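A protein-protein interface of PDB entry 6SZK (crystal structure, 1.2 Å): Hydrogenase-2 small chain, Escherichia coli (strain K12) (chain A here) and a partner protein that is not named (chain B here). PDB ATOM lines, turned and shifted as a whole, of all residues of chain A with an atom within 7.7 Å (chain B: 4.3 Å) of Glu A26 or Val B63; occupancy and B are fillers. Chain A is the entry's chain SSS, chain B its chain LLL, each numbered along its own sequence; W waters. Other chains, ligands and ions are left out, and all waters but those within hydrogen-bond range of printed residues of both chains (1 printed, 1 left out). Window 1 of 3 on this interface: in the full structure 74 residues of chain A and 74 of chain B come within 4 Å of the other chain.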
ATOM      1  N   TRP A  15      12.617 -18.780  38.657  1.00  0.00           N
ATOM      2  CA  TRP A  15      13.251 -19.375  37.453  1.00  0.00           C
ATOM      3  C   TRP A  15      14.739 -19.628  37.766  1.00  0.00           C
ATOM      4  O   TRP A  15      15.483 -18.671  38.076  1.00  0.00           O
ATOM      5  CB  TRP A  15      13.068 -18.449  36.256  1.00  0.00           C
ATOM      6  CG  TRP A  15      13.575 -18.987  34.936  1.00  0.00           C
ATOM      7  CD1 TRP A  15      14.830 -19.488  34.617  1.00  0.00           C
ATOM      8  CD2 TRP A  15      12.799 -19.068  33.704  1.00  0.00           C
ATOM      9  NE1 TRP A  15      14.857 -19.874  33.293  1.00  0.00           N
ATOM     10  CE2 TRP A  15      13.640 -19.600  32.712  1.00  0.00           C
ATOM     11  CE3 TRP A  15      11.481 -18.638  33.378  1.00  0.00           C
ATOM     12  CZ2 TRP A  15      13.197 -19.816  31.391  1.00  0.00           C
ATOM     13  CZ3 TRP A  15      11.069 -18.838  32.048  1.00  0.00           C
ATOM     14  CH2 TRP A  15      11.911 -19.413  31.092  1.00  0.00           C
ATOM     15  N   CYS A  21      21.686 -22.966  27.815  1.00  0.00           N
ATOM     16  CA  CYS A  21      22.308 -22.081  26.829  1.00  0.00           C
ATOM     17  C   CYS A  21      21.664 -20.645  26.783  1.00  0.00           C
ATOM     18  O   CYS A  21      22.160 -19.771  26.062  1.00  0.00           O
ATOM     19  CB  CYS A  21      22.279 -22.653  25.385  1.00  0.00           C
ATOM     20  SG  CYS A  21      20.692 -22.512  24.536  1.00  0.00           S
ATOM     21  N   THR A  22      20.526 -20.499  27.519  1.00  0.00           N
ATOM     22  CA  THR A  22      19.683 -19.244  27.620  1.00  0.00           C
ATOM     23  C   THR A  22      18.668 -19.133  26.489  1.00  0.00           C
ATOM     24  O   THR A  22      17.821 -18.223  26.519  1.00  0.00           O
ATOM     25  CB  THR A  22      20.546 -17.999  27.895  1.00  0.00           C
ATOM     26  OG1 THR A  22      21.489 -18.314  28.936  1.00  0.00           O
ATOM     27  CG2 THR A  22      19.761 -16.758  28.324  1.00  0.00           C
ATOM     28  N   GLY A  23      18.717 -20.023  25.464  1.00  0.00           N
ATOM     29  CA  GLY A  23      17.699 -20.001  24.429  1.00  0.00           C
ATOM     30  C   GLY A  23      16.261 -20.141  24.920  1.00  0.00           C
ATOM     31  O   GLY A  23      15.332 -19.558  24.257  1.00  0.00           O
ATOM     32  N   CYS A  24      16.016 -20.842  26.009  1.00  0.00           N
ATOM     33  CA  CYS A  24      14.648 -21.013  26.534  1.00  0.00           C
ATOM     34  C   CYS A  24      14.152 -19.672  27.140  1.00  0.00           C
ATOM     35  O   CYS A  24      12.969 -19.293  26.943  1.00  0.00           O
ATOM     36  CB  CYS A  24      14.577 -22.188  27.510  1.00  0.00           C
ATOM     37  SG  CYS A  24      14.715 -23.858  26.747  1.00  0.00           S
ATOM     38  N   THR A  25      14.977 -18.908  27.867  1.00  0.00           N
ATOM     39  CA  THR A  25      14.631 -17.519  28.260  1.00  0.00           C
ATOM     40  C   THR A  25      14.451 -16.641  27.023  1.00  0.00           C
ATOM     41  O   THR A  25      13.484 -15.815  26.955  1.00  0.00           O
ATOM     42  CB  THR A  25      15.678 -16.954  29.224  1.00  0.00           C
ATOM     43  OG1 THR A  25      15.565 -17.642  30.507  1.00  0.00           O
ATOM     44  CG2 THR A  25      15.494 -15.433  29.430  1.00  0.00           C
ATOM     45  N   GLU A  26      15.379 -16.740  26.070  1.00  0.00           N
ATOM     46  CA  GLU A  26      15.318 -15.897  24.872  1.00  0.00           C
ATOM     47  C   GLU A  26      14.015 -16.120  24.051  1.00  0.00           C
ATOM     48  O   GLU A  26      13.543 -15.160  23.404  1.00  0.00           O
ATOM     49  CB  GLU A  26      16.572 -16.117  23.991  1.00  0.00           C
ATOM     50  CG  GLU A  26      17.812 -15.416  24.499  1.00  0.00           C
ATOM     51  CD  GLU A  26      17.875 -13.937  24.205  1.00  0.00           C
ATOM     52  OE1 GLU A  26      16.954 -13.319  23.598  1.00  0.00           O
ATOM     53  OE2 GLU A  26      18.934 -13.306  24.658  1.00  0.00           O
ATOM     54  N   SER A  27      13.421 -17.317  24.113  1.00  0.00           N
ATOM     55  CA  SER A  27      12.144 -17.542  23.424  1.00  0.00           C
ATOM     56  C   SER A  27      11.114 -16.505  23.884  1.00  0.00           C
ATOM     57  O   SER A  27      10.259 -16.034  23.083  1.00  0.00           O
ATOM     58  CB  SER A  27      11.630 -18.981  23.617  1.00  0.00           C
ATOM     59  OG  SER A  27      11.055 -19.228  24.899  1.00  0.00           O
ATOM     60  N   LEU A  28      11.143 -16.115  25.165  1.00  0.00           N
ATOM     61  CA  LEU A  28      10.154 -15.147  25.705  1.00  0.00           C
ATOM     62  C   LEU A  28      10.266 -13.810  25.006  1.00  0.00           C
ATOM     63  O   LEU A  28       9.235 -13.064  24.958  1.00  0.00           O
ATOM     64  CB  LEU A  28      10.357 -14.952  27.222  1.00  0.00           C
ATOM     65  CG  LEU A  28      10.238 -16.173  28.124  1.00  0.00           C
ATOM     66  CD1 LEU A  28      10.469 -15.795  29.590  1.00  0.00           C
ATOM     67  CD2 LEU A  28       8.918 -16.904  27.961  1.00  0.00           C
ATOM     68  N   LEU A  29      11.443 -13.426  24.525  1.00  0.00           N
ATOM     69  CA  LEU A  29      11.651 -12.129  23.807  1.00  0.00           C
ATOM     70  C   LEU A  29      11.024 -12.096  22.398  1.00  0.00           C
ATOM     71  O   LEU A  29      10.954 -11.001  21.791  1.00  0.00           O
ATOM     72  CB  LEU A  29      13.127 -11.704  23.804  1.00  0.00           C
ATOM     73  CG  LEU A  29      13.609 -10.937  25.052  1.00  0.00           C
ATOM     74  CD1 LEU A  29      13.489 -11.690  26.341  1.00  0.00           C
ATOM     75  CD2 LEU A  29      15.039 -10.427  24.829  1.00  0.00           C
ATOM     76  N   ARG A  30      10.589 -13.258  21.879  1.00  0.00           N
ATOM     77  CA  ARG A  30       9.840 -13.361  20.606  1.00  0.00           C
ATOM     78  C   ARG A  30       8.313 -13.389  20.862  1.00  0.00           C
ATOM     79  O   ARG A  30       7.526 -13.229  19.875  1.00  0.00           O
ATOM     80  CB  ARG A  30      10.239 -14.570  19.752  1.00  0.00           C
ATOM     81  CG  ARG A  30      11.652 -14.532  19.155  1.00  0.00           C
ATOM     82  CD  ARG A  30      12.795 -14.611  20.140  1.00  0.00           C
ATOM     83  NE  ARG A  30      14.076 -14.908  19.499  1.00  0.00           N
ATOM     84  CZ  ARG A  30      15.249 -14.655  20.085  1.00  0.00           C
ATOM     85  NH1 ARG A  30      15.348 -14.116  21.271  1.00  0.00           N
ATOM     86  NH2 ARG A  30      16.344 -14.979  19.394  1.00  0.00           N
ATOM     87  N   ALA A  31       7.859 -13.669  22.098  1.00  0.00           N
ATOM     88  CA  ALA A  31       6.432 -13.867  22.389  1.00  0.00           C
ATOM     89  C   ALA A  31       5.614 -12.596  22.140  1.00  0.00           C
ATOM     90  O   ALA A  31       6.099 -11.467  22.314  1.00  0.00           O
ATOM     91  CB  ALA A  31       6.260 -14.321  23.850  1.00  0.00           C
ATOM     92  N   VAL A  36       6.983 -10.149  26.583  1.00  0.00           N
ATOM     93  CA  VAL A  36       7.751 -10.338  27.868  1.00  0.00           C
ATOM     94  C   VAL A  36       7.504  -9.147  28.843  1.00  0.00           C
ATOM     95  O   VAL A  36       7.414  -9.373  30.078  1.00  0.00           O
ATOM     96  CB  VAL A  36       9.264 -10.533  27.592  1.00  0.00           C
ATOM     97  CG1 VAL A  36       9.950  -9.330  26.959  1.00  0.00           C
ATOM     98  CG2 VAL A  36       9.985 -10.982  28.848  1.00  0.00           C
ATOM     99  N   HIS A  49      15.082 -14.283  38.510  1.00  0.00           N
ATOM    100  CA  HIS A  49      15.514 -14.596  37.134  1.00  0.00           C
ATOM    101  C   HIS A  49      16.844 -13.863  36.925  1.00  0.00           C
ATOM    102  O   HIS A  49      16.849 -12.627  36.771  1.00  0.00           O
ATOM    103  CB  HIS A  49      14.464 -14.175  36.052  1.00  0.00           C
ATOM    104  CG  HIS A  49      14.754 -14.912  34.765  1.00  0.00           C
ATOM    105  ND1 HIS A  49      16.069 -14.913  34.208  1.00  0.00           N
ATOM    106  CD2 HIS A  49      13.997 -15.744  34.005  1.00  0.00           C
ATOM    107  CE1 HIS A  49      15.996 -15.775  33.151  1.00  0.00           C
ATOM    108  NE2 HIS A  49      14.759 -16.239  32.977  1.00  0.00           N
ATOM    109  N   VAL A  51      18.900 -13.487  34.468  1.00  0.00           N
ATOM    110  CA  VAL A  51      19.150 -12.768  33.180  1.00  0.00           C
ATOM    111  C   VAL A  51      18.715 -11.303  33.269  1.00  0.00           C
ATOM    112  O   VAL A  51      19.343 -10.415  32.654  1.00  0.00           O
ATOM    113  CB  VAL A  51      18.520 -13.452  31.966  1.00  0.00           C
ATOM    114  CG1 VAL A  51      18.693 -12.654  30.673  1.00  0.00           C
ATOM    115  CG2 VAL A  51      19.155 -14.842  31.767  1.00  0.00           C
ATOM    116  N   ASP A  80      15.421 -24.339  33.237  1.00  0.00           N
ATOM    117  CA  ASP A  80      16.004 -24.664  31.922  1.00  0.00           C
ATOM    118  C   ASP A  80      17.428 -25.231  32.121  1.00  0.00           C
ATOM    119  O   ASP A  80      18.140 -24.919  33.109  1.00  0.00           O
ATOM    120  CB  ASP A  80      15.998 -23.429  30.947  1.00  0.00           C
ATOM    121  CG  ASP A  80      16.667 -22.137  31.430  1.00  0.00           C
ATOM    122  OD1 ASP A  80      16.847 -21.960  32.649  1.00  0.00           O
ATOM    123  OD2 ASP A  80      16.936 -21.250  30.543  1.00  0.00           O
ATOM    124  N   PRO A 154      14.676 -24.130  21.386  1.00  0.00           N
ATOM    125  CA  PRO A 154      13.679 -24.107  22.483  1.00  0.00           C
ATOM    126  C   PRO A 154      12.233 -24.292  21.962  1.00  0.00           C
ATOM    127  O   PRO A 154      11.981 -24.110  20.730  1.00  0.00           O
ATOM    128  CB  PRO A 154      13.823 -22.676  23.051  1.00  0.00           C
ATOM    129  CG  PRO A 154      14.131 -21.845  21.787  1.00  0.00           C
ATOM    130  CD  PRO A 154      14.951 -22.771  20.880  1.00  0.00           C
ATOM    131  N   PRO A 155      11.261 -24.624  22.850  1.00  0.00           N
ATOM    132  CA  PRO A 155       9.864 -24.625  22.389  1.00  0.00           C
ATOM    133  C   PRO A 155       9.401 -23.249  21.887  1.00  0.00           C
ATOM    134  O   PRO A 155       9.935 -22.183  22.303  1.00  0.00           O
ATOM    135  CB  PRO A 155       9.109 -25.012  23.681  1.00  0.00           C
ATOM    136  CG  PRO A 155       9.966 -24.481  24.815  1.00  0.00           C
ATOM    137  CD  PRO A 155      11.389 -24.766  24.299  1.00  0.00           C
ATOM    138  N   PRO A 157       7.488 -20.135  22.639  1.00  0.00           N
ATOM    139  CA  PRO A 157       7.290 -19.665  24.023  1.00  0.00           C
ATOM    140  C   PRO A 157       5.853 -19.813  24.527  1.00  0.00           C
ATOM    141  O   PRO A 157       5.635 -19.909  25.765  1.00  0.00           O
ATOM    142  CB  PRO A 157       7.705 -18.172  23.988  1.00  0.00           C
ATOM    143  CG  PRO A 157       7.546 -17.814  22.509  1.00  0.00           C
ATOM    144  CD  PRO A 157       7.938 -19.053  21.721  1.00  0.00           C
ATOM    145  N   GLU B  14      24.738 -13.519  30.156  1.00  0.00           N
ATOM    146  CA  GLU B  14      24.463 -14.931  29.857  1.00  0.00           C
ATOM    147  C   GLU B  14      25.327 -15.836  30.711  1.00  0.00           C
ATOM    148  O   GLU B  14      26.575 -15.718  30.737  1.00  0.00           O
ATOM    149  CB  GLU B  14      24.629 -15.248  28.354  1.00  0.00           C
ATOM    150  CG  GLU B  14      24.107 -16.625  27.921  1.00  0.00           C
ATOM    151  CD  GLU B  14      24.756 -17.819  28.564  1.00  0.00           C
ATOM    152  OE1 GLU B  14      25.970 -17.827  28.782  1.00  0.00           O
ATOM    153  OE2 GLU B  14      24.027 -18.880  28.841  1.00  0.00           O
ATOM    154  N   CYS B  61      25.220 -21.627  22.648  1.00  0.00           N
ATOM    155  CA  CYS B  61      24.599 -20.398  23.205  1.00  0.00           C
ATOM    156  C   CYS B  61      23.322 -20.037  22.461  1.00  0.00           C
ATOM    157  O   CYS B  61      23.309 -20.005  21.207  1.00  0.00           O
ATOM    158  CB  CYS B  61      25.605 -19.239  23.143  1.00  0.00           C
ATOM    159  SG  CYS B  61      25.041 -17.744  24.007  1.00  0.00           S
ATOM    160  N   GLY B  62      22.289 -19.667  23.254  1.00  0.00           N
ATOM    161  CA  GLY B  62      21.042 -19.167  22.700  1.00  0.00           C
ATOM    162  C   GLY B  62      20.878 -17.662  22.726  1.00  0.00           C
ATOM    163  O   GLY B  62      19.863 -17.159  22.162  1.00  0.00           O
ATOM    164  N   VAL B  63      21.776 -16.918  23.411  1.00  0.00           N
ATOM    165  CA  VAL B  63      21.811 -15.456  23.298  1.00  0.00           C
ATOM    166  C   VAL B  63      22.449 -15.119  21.939  1.00  0.00           C
ATOM    167  O   VAL B  63      21.778 -14.521  21.041  1.00  0.00           O
ATOM    168  CB  VAL B  63      22.514 -14.733  24.478  1.00  0.00           C
ATOM    169  CG1 VAL B  63      22.536 -13.208  24.192  1.00  0.00           C
ATOM    170  CG2 VAL B  63      21.756 -15.064  25.771  1.00  0.00           C
ATOM    171  N   CYS B  64      23.678 -15.571  21.722  1.00  0.00           N
ATOM    172  CA  CYS B  64      24.356 -15.456  20.397  1.00  0.00           C
ATOM    173  C   CYS B  64      24.014 -16.689  19.568  1.00  0.00           C
ATOM    174  O   CYS B  64      24.854 -17.344  18.929  1.00  0.00           O
ATOM    175  CB  CYS B  64      25.861 -15.181  20.562  1.00  0.00           C
ATOM    176  SG  CYS B  64      26.819 -16.495  21.302  1.00  0.00           S
ATOM    177  N   THR B  65      22.690 -16.969  19.465  1.00  0.00           N
ATOM    178  CA  THR B  65      22.169 -17.957  18.489  1.00  0.00           C
ATOM    179  C   THR B  65      22.596 -17.491  17.064  1.00  0.00           C
ATOM    180  O   THR B  65      22.984 -16.307  16.879  1.00  0.00           O
ATOM    181  CB  THR B  65      20.665 -18.203  18.698  1.00  0.00           C
ATOM    182  OG1 THR B  65      20.261 -19.318  17.876  1.00  0.00           O
ATOM    183  CG2 THR B  65      19.808 -17.006  18.303  1.00  0.00           C
ATOM    184  N   HIS B  99      20.325 -10.601  13.482  1.00  0.00           N
ATOM    185  CA  HIS B  99      20.538 -11.180  14.829  1.00  0.00           C
ATOM    186  C   HIS B  99      21.377 -10.219  15.718  1.00  0.00           C
ATOM    187  O   HIS B  99      21.002  -9.932  16.900  1.00  0.00           O
ATOM    188  CB  HIS B  99      21.258 -12.565  14.769  1.00  0.00           C
ATOM    189  CG  HIS B  99      21.612 -12.967  16.181  1.00  0.00           C
ATOM    190  ND1 HIS B  99      20.690 -13.468  17.058  1.00  0.00           N
ATOM    191  CD2 HIS B  99      22.746 -12.662  16.896  1.00  0.00           C
ATOM    192  CE1 HIS B  99      21.258 -13.529  18.272  1.00  0.00           C
ATOM    193  NE2 HIS B  99      22.495 -12.954  18.220  1.00  0.00           N
ATOM    194  N   HIS B 102      19.363  -7.247  17.186  1.00  0.00           N
ATOM    195  CA  HIS B 102      18.646  -7.680  18.423  1.00  0.00           C
ATOM    196  C   HIS B 102      19.600  -7.768  19.580  1.00  0.00           C
ATOM    197  O   HIS B 102      19.281  -7.311  20.721  1.00  0.00           O
ATOM    198  CB  HIS B 102      17.935  -9.032  18.141  1.00  0.00           C
ATOM    199  CG  HIS B 102      17.886  -9.998  19.285  1.00  0.00           C
ATOM    200  ND1 HIS B 102      16.914 -10.024  20.308  1.00  0.00           N
ATOM    201  CD2 HIS B 102      18.734 -11.033  19.586  1.00  0.00           C
ATOM    202  CE1 HIS B 102      17.240 -11.005  21.180  1.00  0.00           C
ATOM    203  NE2 HIS B 102      18.332 -11.639  20.767  1.00  0.00           N
ATOM    204  N   ASP B 103      20.759  -8.421  19.378  1.00  0.00           N
ATOM    205  CA  ASP B 103      21.681  -8.750  20.490  1.00  0.00           C
ATOM    206  C   ASP B 103      22.217  -7.443  21.153  1.00  0.00           C
ATOM    207  O   ASP B 103      22.159  -7.284  22.401  1.00  0.00           O
ATOM    208  CB  ASP B 103      22.815  -9.577  19.864  1.00  0.00           C
ATOM    209  CG  ASP B 103      23.613 -10.448  20.746  1.00  0.00           C
ATOM    210  OD1 ASP B 103      24.134  -9.821  21.726  1.00  0.00           O
ATOM    211  OD2 ASP B 103      23.888 -11.664  20.406  1.00  0.00           O
ATOM    212  N   PRO B 213      14.748 -18.468  18.783  1.00  0.00           N
ATOM    213  CA  PRO B 213      16.152 -18.940  18.801  1.00  0.00           C
ATOM    214  C   PRO B 213      16.388 -20.265  18.013  1.00  0.00           C
ATOM    215  O   PRO B 213      15.496 -21.099  17.862  1.00  0.00           O
ATOM    216  CB  PRO B 213      16.512 -19.129  20.275  1.00  0.00           C
ATOM    217  CG  PRO B 213      15.463 -18.280  21.027  1.00  0.00           C
ATOM    218  CD  PRO B 213      14.217 -18.394  20.171  1.00  0.00           C
HETATM  219  O   HOH W   1      19.473 -11.014  23.590  1.00  0.00           O
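O of Cys A24 is in hydrogen-bond range of OG of Ser A27 (2.8 Å).
OE1 of Glu A26 lies within salt-bridge range of NH1 of Arg A30 (2.9 Å).
The backbone carbonyl oxygen (O) of Val B63 lies close to a ring nitrogen (NE2) of His B99 (3.3 Å).
The side-chain sulfur (SG) of Cys A21 sits close to the backbone NH (N) of Gly A23 (3.3 Å).
The side-chain sulfur (SG) of Cys B61 lies close to the backbone NH (N) of Val B63 (3.4 Å).
Of the printed residues of chain B, Glu A26 touches Gly B62 (3.6 Å), Val B63 (3.5 Å), His B102 (3.4 Å) and Pro B213 (3.8 Å).
Val B63 touches just these residues of chain A: Cys A21, Thr A22 and Glu A26.
Of the printed residues of chain A, Glu B14 touches Cys A21 and Thr A22.
Of the printed residues of chain A, Cys B61 touches Cys A21.
Printed residues of chain A within 4 Å of Pro B213: Gly A23, Glu A26, Ser A27, Arg A30 and Pro A154.
Cys B64 touches none of the printed residues of chain A.
Pro A155 touches none of the printed residues of chain B.
The nearest printed residue of chain B that does not touch Glu A26 is Cys B64 (6.0 Å).
The nearest residue of chain A that does not touch Val B63 is Gly A23 (4.8 Å).
The nearest printed residue of chain B that does not touch Thr A22 is Gly B62 (4.5 Å).
OE2 of Glu B14 lies within hydrogen-bond range of OG1 of Thr A22 (2.6 Å).
OE2 of Glu B14 lies close to O of Cys A21, at 3.5 Å.
O of Cys A21 is in hydrogen-bond range of N of Gly B62 (2.8 Å).
Among the printed residues, pairs that only touch across the chains: Glu A26 with His B102 (3.4 Å), Gly A23 with Pro B213 (3.5 Å), Pro A154 with Pro B213 (3.5 Å), Glu A26 with Val B63 (3.5 Å), Arg A30 with Pro B213 (3.6 Å), Glu A26 with Gly B62 (3.6 Å), Arg A30 with His B102 (3.6 Å), Thr A22 with Val B63 (3.7 Å), Gly A23 with Gly B62 (3.7 Å), Cys A21 with Cys B61 (3.8 Å), Ser A27 with Pro B213 (3.8 Å), Glu A26 with Pro B213 (3.8 Å) and Cys A21 with Val B63 (3.9 Å).
Of the 10 printed residues of chain B, 6 touch a printed residue of chain A.
Hydrophobic or aromatic side chains of chain B that line the printed part of chain A: Val B63, His B102 and Pro B213.
Of the 19 printed residues of chain A, 7 touch a printed residue of chain B.
Printed residues of chain A that touch a printed residue of chain B: Cys A21, Thr A22, Gly A23, Glu A26, Ser A27, Arg A30 and Pro A154.
Hydrophobic or aromatic side chains of chain A that line the printed part of chain B: Pro A154.
Among the printed residues, 16 pairs touch across the chains.
Among the printed residues, no Asp or Glu carboxylate lies within 4 Å of a Lys or Arg side-chain nitrogen of the other chain.
Water W1 lies within hydrogen-bond range of the side-chain carboxylate of Glu A26 (2.6 Å) and a ring nitrogen (NE2) of His B102 (3.1 Å).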
